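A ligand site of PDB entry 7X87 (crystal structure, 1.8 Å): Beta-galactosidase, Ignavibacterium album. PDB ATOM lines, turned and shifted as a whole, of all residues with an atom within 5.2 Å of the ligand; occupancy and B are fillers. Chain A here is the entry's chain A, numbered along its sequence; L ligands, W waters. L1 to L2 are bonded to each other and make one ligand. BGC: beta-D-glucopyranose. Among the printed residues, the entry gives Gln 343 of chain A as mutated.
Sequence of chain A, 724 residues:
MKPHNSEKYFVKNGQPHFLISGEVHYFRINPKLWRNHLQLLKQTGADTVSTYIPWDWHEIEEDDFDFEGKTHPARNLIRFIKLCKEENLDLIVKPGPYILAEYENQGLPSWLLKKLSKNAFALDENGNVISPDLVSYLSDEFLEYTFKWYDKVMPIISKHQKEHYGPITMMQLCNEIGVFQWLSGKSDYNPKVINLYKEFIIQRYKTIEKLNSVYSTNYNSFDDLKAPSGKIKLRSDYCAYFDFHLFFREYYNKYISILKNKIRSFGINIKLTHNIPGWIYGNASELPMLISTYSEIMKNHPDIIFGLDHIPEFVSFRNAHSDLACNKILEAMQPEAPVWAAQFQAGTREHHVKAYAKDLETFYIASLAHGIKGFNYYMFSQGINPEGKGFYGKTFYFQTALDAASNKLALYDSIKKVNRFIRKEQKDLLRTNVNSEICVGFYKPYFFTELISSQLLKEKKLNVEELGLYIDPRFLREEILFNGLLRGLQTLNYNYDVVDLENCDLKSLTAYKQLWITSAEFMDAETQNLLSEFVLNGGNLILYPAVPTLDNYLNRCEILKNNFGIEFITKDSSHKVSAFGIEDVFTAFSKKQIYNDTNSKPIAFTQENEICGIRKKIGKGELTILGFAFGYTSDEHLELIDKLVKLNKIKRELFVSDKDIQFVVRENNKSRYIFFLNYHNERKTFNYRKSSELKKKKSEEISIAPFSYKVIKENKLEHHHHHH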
ATOM      1  N   LEU A 100     -25.315 -25.043  24.690  1.00  0.00           N
ATOM      2  CA  LEU A 100     -25.402 -26.440  24.209  1.00  0.00           C
ATOM      3  C   LEU A 100     -24.094 -26.734  23.469  1.00  0.00           C
ATOM      4  O   LEU A 100     -23.095 -26.939  24.183  1.00  0.00           O
ATOM      5  CB  LEU A 100     -26.642 -26.662  23.339  1.00  0.00           C
ATOM      6  CG  LEU A 100     -27.924 -26.914  24.137  1.00  0.00           C
ATOM      7  CD1 LEU A 100     -28.287 -25.713  24.994  1.00  0.00           C
ATOM      8  CD2 LEU A 100     -29.055 -27.295  23.222  1.00  0.00           C
ATOM      9  N   ALA A 101     -24.092 -26.701  22.146  1.00  0.00           N
ATOM     10  CA  ALA A 101     -22.858 -26.650  21.304  1.00  0.00           C
ATOM     11  C   ALA A 101     -21.958 -27.865  21.587  1.00  0.00           C
ATOM     12  O   ALA A 101     -20.736 -27.771  21.375  1.00  0.00           O
ATOM     13  CB  ALA A 101     -22.130 -25.368  21.587  1.00  0.00           C
ATOM     14  N   GLU A 102     -22.530 -28.993  22.025  1.00  0.00           N
ATOM     15  CA  GLU A 102     -21.747 -30.187  22.448  1.00  0.00           C
ATOM     16  C   GLU A 102     -20.621 -29.789  23.384  1.00  0.00           C
ATOM     17  O   GLU A 102     -19.549 -30.358  23.265  1.00  0.00           O
ATOM     18  CB  GLU A 102     -21.135 -30.880  21.231  1.00  0.00           C
ATOM     19  CG  GLU A 102     -22.164 -31.519  20.332  1.00  0.00           C
ATOM     20  CD  GLU A 102     -21.597 -32.725  19.608  1.00  0.00           C
ATOM     21  OE1 GLU A 102     -20.326 -32.909  19.604  1.00  0.00           O
ATOM     22  OE2 GLU A 102     -22.412 -33.495  19.081  1.00  0.00           O
ATOM     23  N   TYR A 103     -20.858 -28.825  24.275  1.00  0.00           N
ATOM     24  CA  TYR A 103     -19.899 -28.381  25.309  1.00  0.00           C
ATOM     25  C   TYR A 103     -20.352 -29.009  26.629  1.00  0.00           C
ATOM     26  O   TYR A 103     -21.579 -29.091  26.838  1.00  0.00           O
ATOM     27  CB  TYR A 103     -19.912 -26.850  25.360  1.00  0.00           C
ATOM     28  CG  TYR A 103     -18.796 -26.230  26.147  1.00  0.00           C
ATOM     29  CD1 TYR A 103     -18.781 -26.269  27.518  1.00  0.00           C
ATOM     30  CD2 TYR A 103     -17.770 -25.568  25.502  1.00  0.00           C
ATOM     31  CE1 TYR A 103     -17.782 -25.677  28.251  1.00  0.00           C
ATOM     32  CE2 TYR A 103     -16.761 -24.944  26.220  1.00  0.00           C
ATOM     33  CZ  TYR A 103     -16.769 -24.985  27.587  1.00  0.00           C
ATOM     34  OH  TYR A 103     -15.800 -24.410  28.336  1.00  0.00           O
ATOM     35  N   GLN A 106     -23.520 -28.156  28.814  1.00  0.00           N
ATOM     36  CA  GLN A 106     -24.185 -27.265  27.830  1.00  0.00           C
ATOM     37  C   GLN A 106     -23.601 -25.855  27.930  1.00  0.00           C
ATOM     38  O   GLN A 106     -24.319 -24.914  27.548  1.00  0.00           O
ATOM     39  CB  GLN A 106     -25.683 -27.201  28.110  1.00  0.00           C
ATOM     40  CG  GLN A 106     -26.294 -28.575  28.377  1.00  0.00           C
ATOM     41  CD  GLN A 106     -26.019 -29.521  27.238  1.00  0.00           C
ATOM     42  OE1 GLN A 106     -25.846 -29.119  26.081  1.00  0.00           O
ATOM     43  NE2 GLN A 106     -26.008 -30.796  27.546  1.00  0.00           N
ATOM     44  N   GLU A 176     -31.825 -22.094  21.911  1.00  0.00           N
ATOM     45  CA  GLU A 176     -32.935 -23.084  21.717  1.00  0.00           C
ATOM     46  C   GLU A 176     -33.737 -23.285  23.012  1.00  0.00           C
ATOM     47  O   GLU A 176     -33.784 -24.432  23.564  1.00  0.00           O
ATOM     48  CB  GLU A 176     -32.367 -24.416  21.203  1.00  0.00           C
ATOM     49  CG  GLU A 176     -31.822 -24.337  19.793  1.00  0.00           C
ATOM     50  CD  GLU A 176     -31.262 -25.639  19.251  1.00  0.00           C
ATOM     51  OE1 GLU A 176     -30.944 -26.528  20.068  1.00  0.00           O
ATOM     52  OE2 GLU A 176     -31.135 -25.749  18.012  1.00  0.00           O
ATOM     53  N   VAL A 179     -35.354 -26.662  24.533  1.00  0.00           N
ATOM     54  CA  VAL A 179     -34.904 -27.851  23.746  1.00  0.00           C
ATOM     55  C   VAL A 179     -34.740 -29.075  24.671  1.00  0.00           C
ATOM     56  O   VAL A 179     -34.879 -30.185  24.173  1.00  0.00           O
ATOM     57  CB  VAL A 179     -33.642 -27.553  22.913  1.00  0.00           C
ATOM     58  CG1 VAL A 179     -32.410 -27.359  23.776  1.00  0.00           C
ATOM     59  CG2 VAL A 179     -33.393 -28.626  21.845  1.00  0.00           C
ATOM     60  N   PHE A 180     -34.541 -28.909  25.994  1.00  0.00           N
ATOM     61  CA  PHE A 180     -34.398 -30.039  26.959  1.00  0.00           C
ATOM     62  C   PHE A 180     -35.746 -30.533  27.510  1.00  0.00           C
ATOM     63  O   PHE A 180     -35.918 -31.747  27.654  1.00  0.00           O
ATOM     64  CB  PHE A 180     -33.487 -29.629  28.103  1.00  0.00           C
ATOM     65  CG  PHE A 180     -32.081 -29.279  27.678  1.00  0.00           C
ATOM     66  CD1 PHE A 180     -31.264 -30.242  27.107  1.00  0.00           C
ATOM     67  CD2 PHE A 180     -31.579 -28.016  27.907  1.00  0.00           C
ATOM     68  CE1 PHE A 180     -29.973 -29.923  26.724  1.00  0.00           C
ATOM     69  CE2 PHE A 180     -30.278 -27.704  27.543  1.00  0.00           C
ATOM     70  CZ  PHE A 180     -29.493 -28.652  26.952  1.00  0.00           C
ATOM     71  N   TRP A 182     -38.084 -30.773  25.646  1.00  0.00           N
ATOM     72  CA  TRP A 182     -38.409 -31.581  24.433  1.00  0.00           C
ATOM     73  C   TRP A 182     -37.612 -32.900  24.427  1.00  0.00           C
ATOM     74  O   TRP A 182     -38.267 -33.966  24.359  1.00  0.00           O
ATOM     75  CB  TRP A 182     -38.166 -30.724  23.167  1.00  0.00           C
ATOM     76  CG  TRP A 182     -38.284 -31.487  21.876  1.00  0.00           C
ATOM     77  CD1 TRP A 182     -39.342 -32.251  21.478  1.00  0.00           C
ATOM     78  CD2 TRP A 182     -37.310 -31.542  20.812  1.00  0.00           C
ATOM     79  NE1 TRP A 182     -39.079 -32.772  20.234  1.00  0.00           N
ATOM     80  CE2 TRP A 182     -37.860 -32.345  19.799  1.00  0.00           C
ATOM     81  CE3 TRP A 182     -36.061 -30.963  20.596  1.00  0.00           C
ATOM     82  CZ2 TRP A 182     -37.190 -32.612  18.608  1.00  0.00           C
ATOM     83  CZ3 TRP A 182     -35.399 -31.208  19.412  1.00  0.00           C
ATOM     84  CH2 TRP A 182     -35.957 -32.029  18.441  1.00  0.00           C
ATOM     85  N   LEU A 183     -36.267 -32.810  24.438  1.00  0.00           N
ATOM     86  CA  LEU A 183     -35.304 -33.937  24.241  1.00  0.00           C
ATOM     87  C   LEU A 183     -35.324 -34.902  25.419  1.00  0.00           C
ATOM     88  O   LEU A 183     -35.424 -36.121  25.143  1.00  0.00           O
ATOM     89  CB  LEU A 183     -33.882 -33.428  24.062  1.00  0.00           C
ATOM     90  CG  LEU A 183     -33.557 -32.710  22.747  1.00  0.00           C
ATOM     91  CD1 LEU A 183     -32.143 -32.188  22.791  1.00  0.00           C
ATOM     92  CD2 LEU A 183     -33.738 -33.615  21.539  1.00  0.00           C
ATOM     93  N   ILE A 276     -34.158 -21.737  16.530  1.00  0.00           N
ATOM     94  CA  ILE A 276     -35.251 -22.724  16.611  1.00  0.00           C
ATOM     95  C   ILE A 276     -34.730 -24.142  16.372  1.00  0.00           C
ATOM     96  O   ILE A 276     -34.254 -24.470  15.266  1.00  0.00           O
ATOM     97  CB  ILE A 276     -36.344 -22.333  15.596  1.00  0.00           C
ATOM     98  CG1 ILE A 276     -36.853 -20.907  15.783  1.00  0.00           C
ATOM     99  CG2 ILE A 276     -37.482 -23.338  15.717  1.00  0.00           C
ATOM    100  CD1 ILE A 276     -37.530 -20.351  14.522  1.00  0.00           C
ATOM    101  N   PRO A 277     -34.862 -25.037  17.397  1.00  0.00           N
ATOM    102  CA  PRO A 277     -34.524 -26.447  17.254  1.00  0.00           C
ATOM    103  C   PRO A 277     -35.644 -27.214  16.552  1.00  0.00           C
ATOM    104  O   PRO A 277     -36.755 -26.664  16.358  1.00  0.00           O
ATOM    105  CB  PRO A 277     -34.438 -26.885  18.734  1.00  0.00           C
ATOM    106  CG  PRO A 277     -35.543 -26.074  19.395  1.00  0.00           C
ATOM    107  CD  PRO A 277     -35.458 -24.733  18.698  1.00  0.00           C
ATOM    108  N   GLY A 278     -35.418 -28.495  16.235  1.00  0.00           N
ATOM    109  CA  GLY A 278     -36.533 -29.395  15.852  1.00  0.00           C
ATOM    110  C   GLY A 278     -36.174 -30.397  14.800  1.00  0.00           C
ATOM    111  O   GLY A 278     -36.963 -31.351  14.603  1.00  0.00           O
ATOM    112  N   TRP A 279     -35.023 -30.261  14.149  1.00  0.00           N
ATOM    113  CA  TRP A 279     -34.615 -31.310  13.186  1.00  0.00           C
ATOM    114  C   TRP A 279     -34.080 -32.484  13.998  1.00  0.00           C
ATOM    115  O   TRP A 279     -33.317 -32.261  14.987  1.00  0.00           O
ATOM    116  CB  TRP A 279     -33.566 -30.809  12.213  1.00  0.00           C
ATOM    117  CG  TRP A 279     -34.003 -29.867  11.142  1.00  0.00           C
ATOM    118  CD1 TRP A 279     -34.266 -28.526  11.258  1.00  0.00           C
ATOM    119  CD2 TRP A 279     -34.137 -30.175   9.757  1.00  0.00           C
ATOM    120  NE1 TRP A 279     -34.593 -27.998  10.045  1.00  0.00           N
ATOM    121  CE2 TRP A 279     -34.482 -28.985   9.095  1.00  0.00           C
ATOM    122  CE3 TRP A 279     -33.998 -31.358   9.006  1.00  0.00           C
ATOM    123  CZ2 TRP A 279     -34.703 -28.930   7.722  1.00  0.00           C
ATOM    124  CZ3 TRP A 279     -34.193 -31.304   7.650  1.00  0.00           C
ATOM    125  CH2 TRP A 279     -34.543 -30.109   7.020  1.00  0.00           C
ATOM    126  N   ILE A 280     -34.397 -33.713  13.580  1.00  0.00           N
ATOM    127  CA  ILE A 280     -33.718 -34.902  14.151  1.00  0.00           C
ATOM    128  C   ILE A 280     -33.849 -36.019  13.095  1.00  0.00           C
ATOM    129  O   ILE A 280     -34.858 -36.079  12.432  1.00  0.00           O
ATOM    130  CB  ILE A 280     -34.322 -35.264  15.518  1.00  0.00           C
ATOM    131  CG1 ILE A 280     -33.411 -36.234  16.276  1.00  0.00           C
ATOM    132  CG2 ILE A 280     -35.753 -35.745  15.370  1.00  0.00           C
ATOM    133  CD1 ILE A 280     -33.873 -36.552  17.690  1.00  0.00           C
ATOM    134  N   ASP A 309     -32.550 -23.603  12.887  1.00  0.00           N
ATOM    135  CA  ASP A 309     -31.355 -24.472  13.023  1.00  0.00           C
ATOM    136  C   ASP A 309     -31.547 -25.692  12.113  1.00  0.00           C
ATOM    137  O   ASP A 309     -32.140 -26.687  12.557  1.00  0.00           O
ATOM    138  CB  ASP A 309     -31.083 -24.781  14.500  1.00  0.00           C
ATOM    139  CG  ASP A 309     -30.720 -23.540  15.295  1.00  0.00           C
ATOM    140  OD1 ASP A 309     -30.392 -22.507  14.657  1.00  0.00           O
ATOM    141  OD2 ASP A 309     -30.781 -23.626  16.554  1.00  0.00           O
ATOM    142  N   ILE A 311     -30.758 -28.929  10.073  1.00  0.00           N
ATOM    143  CA  ILE A 311     -29.861 -30.108  10.164  1.00  0.00           C
ATOM    144  C   ILE A 311     -30.422 -31.225   9.270  1.00  0.00           C
ATOM    145  O   ILE A 311     -30.882 -32.262   9.774  1.00  0.00           O
ATOM    146  CB  ILE A 311     -29.638 -30.617  11.598  1.00  0.00           C
ATOM    147  CG1 ILE A 311     -29.466 -29.496  12.632  1.00  0.00           C
ATOM    148  CG2 ILE A 311     -28.460 -31.572  11.622  1.00  0.00           C
ATOM    149  CD1 ILE A 311     -29.406 -30.056  14.028  1.00  0.00           C
ATOM    150  N   GLN A 343     -28.354 -21.475  12.302  1.00  0.00           N
ATOM    151  CA  GLN A 343     -27.407 -22.595  12.178  1.00  0.00           C
ATOM    152  C   GLN A 343     -27.814 -23.333  10.903  1.00  0.00           C
ATOM    153  O   GLN A 343     -28.949 -23.805  10.853  1.00  0.00           O
ATOM    154  CB  GLN A 343     -27.444 -23.524  13.407  1.00  0.00           C
ATOM    155  CG  GLN A 343     -27.045 -22.828  14.686  1.00  0.00           C
ATOM    156  CD  GLN A 343     -27.183 -23.724  15.899  1.00  0.00           C
ATOM    157  OE1 GLN A 343     -27.141 -24.955  15.811  1.00  0.00           O
ATOM    158  NE2 GLN A 343     -27.476 -23.132  17.019  1.00  0.00           N
ATOM    159  N   ARG A 349     -22.146 -32.817  13.122  1.00  0.00           N
ATOM    160  CA  ARG A 349     -21.857 -32.922  14.573  1.00  0.00           C
ATOM    161  C   ARG A 349     -21.487 -34.349  14.988  1.00  0.00           C
ATOM    162  O   ARG A 349     -20.823 -34.509  16.047  1.00  0.00           O
ATOM    163  CB  ARG A 349     -23.105 -32.446  15.326  1.00  0.00           C
ATOM    164  CG  ARG A 349     -24.351 -33.270  15.004  1.00  0.00           C
ATOM    165  CD  ARG A 349     -25.651 -32.669  15.527  1.00  0.00           C
ATOM    166  NE  ARG A 349     -26.819 -33.480  15.150  1.00  0.00           N
ATOM    167  CZ  ARG A 349     -28.025 -33.337  15.684  1.00  0.00           C
ATOM    168  NH1 ARG A 349     -28.209 -32.434  16.630  1.00  0.00           N
ATOM    169  NH2 ARG A 349     -29.027 -34.111  15.310  1.00  0.00           N
ATOM    170  N   PHE A 391     -18.649 -32.466  25.066  1.00  0.00           N
ATOM    171  CA  PHE A 391     -19.697 -33.316  25.674  1.00  0.00           C
ATOM    172  C   PHE A 391     -19.445 -34.806  25.350  1.00  0.00           C
ATOM    173  O   PHE A 391     -19.631 -35.633  26.248  1.00  0.00           O
ATOM    174  CB  PHE A 391     -21.080 -32.866  25.201  1.00  0.00           C
ATOM    175  CG  PHE A 391     -22.196 -33.440  26.030  1.00  0.00           C
ATOM    176  CD1 PHE A 391     -22.680 -34.720  25.800  1.00  0.00           C
ATOM    177  CD2 PHE A 391     -22.736 -32.707  27.081  1.00  0.00           C
ATOM    178  CE1 PHE A 391     -23.672 -35.267  26.592  1.00  0.00           C
ATOM    179  CE2 PHE A 391     -23.747 -33.243  27.850  1.00  0.00           C
ATOM    180  CZ  PHE A 391     -24.190 -34.527  27.634  1.00  0.00           C
ATOM    181  N   TYR A 392     -19.037 -35.126  24.117  1.00  0.00           N
ATOM    182  CA  TYR A 392     -19.061 -36.496  23.536  1.00  0.00           C
ATOM    183  C   TYR A 392     -17.730 -36.987  22.920  1.00  0.00           C
ATOM    184  O   TYR A 392     -17.730 -38.080  22.274  1.00  0.00           O
ATOM    185  CB  TYR A 392     -19.951 -36.581  22.304  1.00  0.00           C
ATOM    186  CG  TYR A 392     -21.426 -36.451  22.555  1.00  0.00           C
ATOM    187  CD1 TYR A 392     -22.105 -37.392  23.315  1.00  0.00           C
ATOM    188  CD2 TYR A 392     -22.146 -35.433  21.948  1.00  0.00           C
ATOM    189  CE1 TYR A 392     -23.458 -37.280  23.537  1.00  0.00           C
ATOM    190  CE2 TYR A 392     -23.520 -35.339  22.132  1.00  0.00           C
ATOM    191  CZ  TYR A 392     -24.178 -36.267  22.907  1.00  0.00           C
ATOM    192  OH  TYR A 392     -25.505 -36.163  23.085  1.00  0.00           O
HETATM  193  C2  BGC L   1     -27.997 -31.368  21.048  1.00  0.00           C
HETATM  194  C3  BGC L   1     -26.770 -30.560  21.369  1.00  0.00           C
HETATM  195  C4  BGC L   1     -26.182 -30.866  22.765  1.00  0.00           C
HETATM  196  C5  BGC L   1     -25.922 -32.365  22.864  1.00  0.00           C
HETATM  197  C6  BGC L   1     -25.450 -32.707  24.279  1.00  0.00           C
HETATM  198  C1  BGC L   1     -27.646 -32.882  21.231  1.00  0.00           C
HETATM  199  O1  BGC L   1     -28.768 -33.798  21.010  1.00  0.00           O
HETATM  200  O2  BGC L   1     -28.286 -31.051  19.645  1.00  0.00           O
HETATM  201  O3  BGC L   1     -27.177 -29.209  21.260  1.00  0.00           O
HETATM  202  O4  BGC L   1     -25.037 -30.028  23.057  1.00  0.00           O
HETATM  203  O5  BGC L   1     -27.152 -33.065  22.584  1.00  0.00           O
HETATM  204  O6  BGC L   1     -26.487 -32.392  25.185  1.00  0.00           O
HETATM  205  C2  BGC L   2     -29.697 -29.507  18.401  1.00  0.00           C
HETATM  206  C3  BGC L   2     -31.110 -29.205  17.912  1.00  0.00           C
HETATM  207  C4  BGC L   2     -31.738 -30.521  17.346  1.00  0.00           C
HETATM  208  C5  BGC L   2     -31.667 -31.595  18.422  1.00  0.00           C
HETATM  209  C6  BGC L   2     -32.123 -32.998  17.964  1.00  0.00           C
HETATM  210  C1  BGC L   2     -29.654 -30.680  19.393  1.00  0.00           C
HETATM  211  O2  BGC L   2     -29.183 -28.337  19.087  1.00  0.00           O
HETATM  212  O3  BGC L   2     -31.050 -28.182  16.931  1.00  0.00           O
HETATM  213  O4  BGC L   2     -33.075 -30.295  16.903  1.00  0.00           O
HETATM  214  O5  BGC L   2     -30.322 -31.843  18.857  1.00  0.00           O
HETATM  215  O6  BGC L   2     -31.480 -33.363  16.726  1.00  0.00           O
HETATM  216  O   HOH W   1     -28.127 -25.008  19.002  1.00  0.00           O
HETATM  217  O   HOH W   2     -32.710 -28.400  14.566  1.00  0.00           O
HETATM  218  O   HOH W   3     -27.620 -27.444  17.431  1.00  0.00           O
HETATM  219  O   HOH W   4     -27.060 -34.816  18.423  1.00  0.00           O
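Water W3 lies within hydrogen-bond range of O2 of BGC L2 (2.4 Å) and OE1 of Gln 343 (3.0 Å). Water W2 lies within hydrogen-bond range of the backbone carbonyl oxygen (O) of Asp 309, an oxygen (O3) of BGC L2, the backbone NH (N) of Trp 279 and the backbone NH (N) of Gly 278. Water W4 bridges NH1 of Arg 349 (3.2 Å) and O1 of BGC L1 (3.3 Å). Water W1 lies within hydrogen-bond range of the side-chain amide nitrogen (NE2) of Gln 343 (2.8 Å), the side-chain carboxylate (OE2) of Glu 176 (3.3 Å) and an oxygen (O2) of BGC L2 (3.5 Å).
Merely in contact with the ligand: Leu 100, Ile 280, Trp 182, Tyr 392, Ala 101, Phe 391, Ile 311, Pro 277 and Leu 183. Hydrophobic or aromatic side chains that line the ligand: Leu 100, Trp 182, Leu 183, Ile 280, Ile 311, Phe 391 and Tyr 392. Of the 21 residues printed, 15 come within 4 Å of the ligand. Along chain A the residues within 4 Å of the ligand span positions 100 to 392.
The side-chain carboxylate of Asp 309 lies close to the side-chain carboxylate of Glu 176, 2.6 Å away. The backbone carbonyl oxygen (O) of Gln 106 is in hydrogen-bond range of the backbone NH (N) of Leu 100 (3.0 Å). O of Glu 102 lies within hydrogen-bond range of N of Phe 391, 2.9 Å away.
An oxygen (O3) of BGC L2 sits at hydrogen-bond distance from the side-chain carboxylate of Glu 176 (2.7 Å). N of Trp 279 sits at hydrogen-bond distance from O4 of BGC L2 (3.4 Å). An oxygen (O4) of BGC L2 sits at hydrogen-bond distance from the backbone carbonyl oxygen (O) of Trp 279 (2.8 Å). NE2 of Gln 106 is in hydrogen-bond range of O6 of BGC L1, 2.9 Å away. The backbone NH (N) of Glu 102 sits at hydrogen-bond distance from an oxygen (O4) of BGC L1 (2.9 Å). An oxygen (O6) of BGC L2 is in hydrogen-bond range of the guanidinium group of Arg 349 (2.9 Å). The backbone NH of Gly 278 sits at hydrogen-bond distance from an oxygen (O4) of BGC L2 (3.0 Å).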
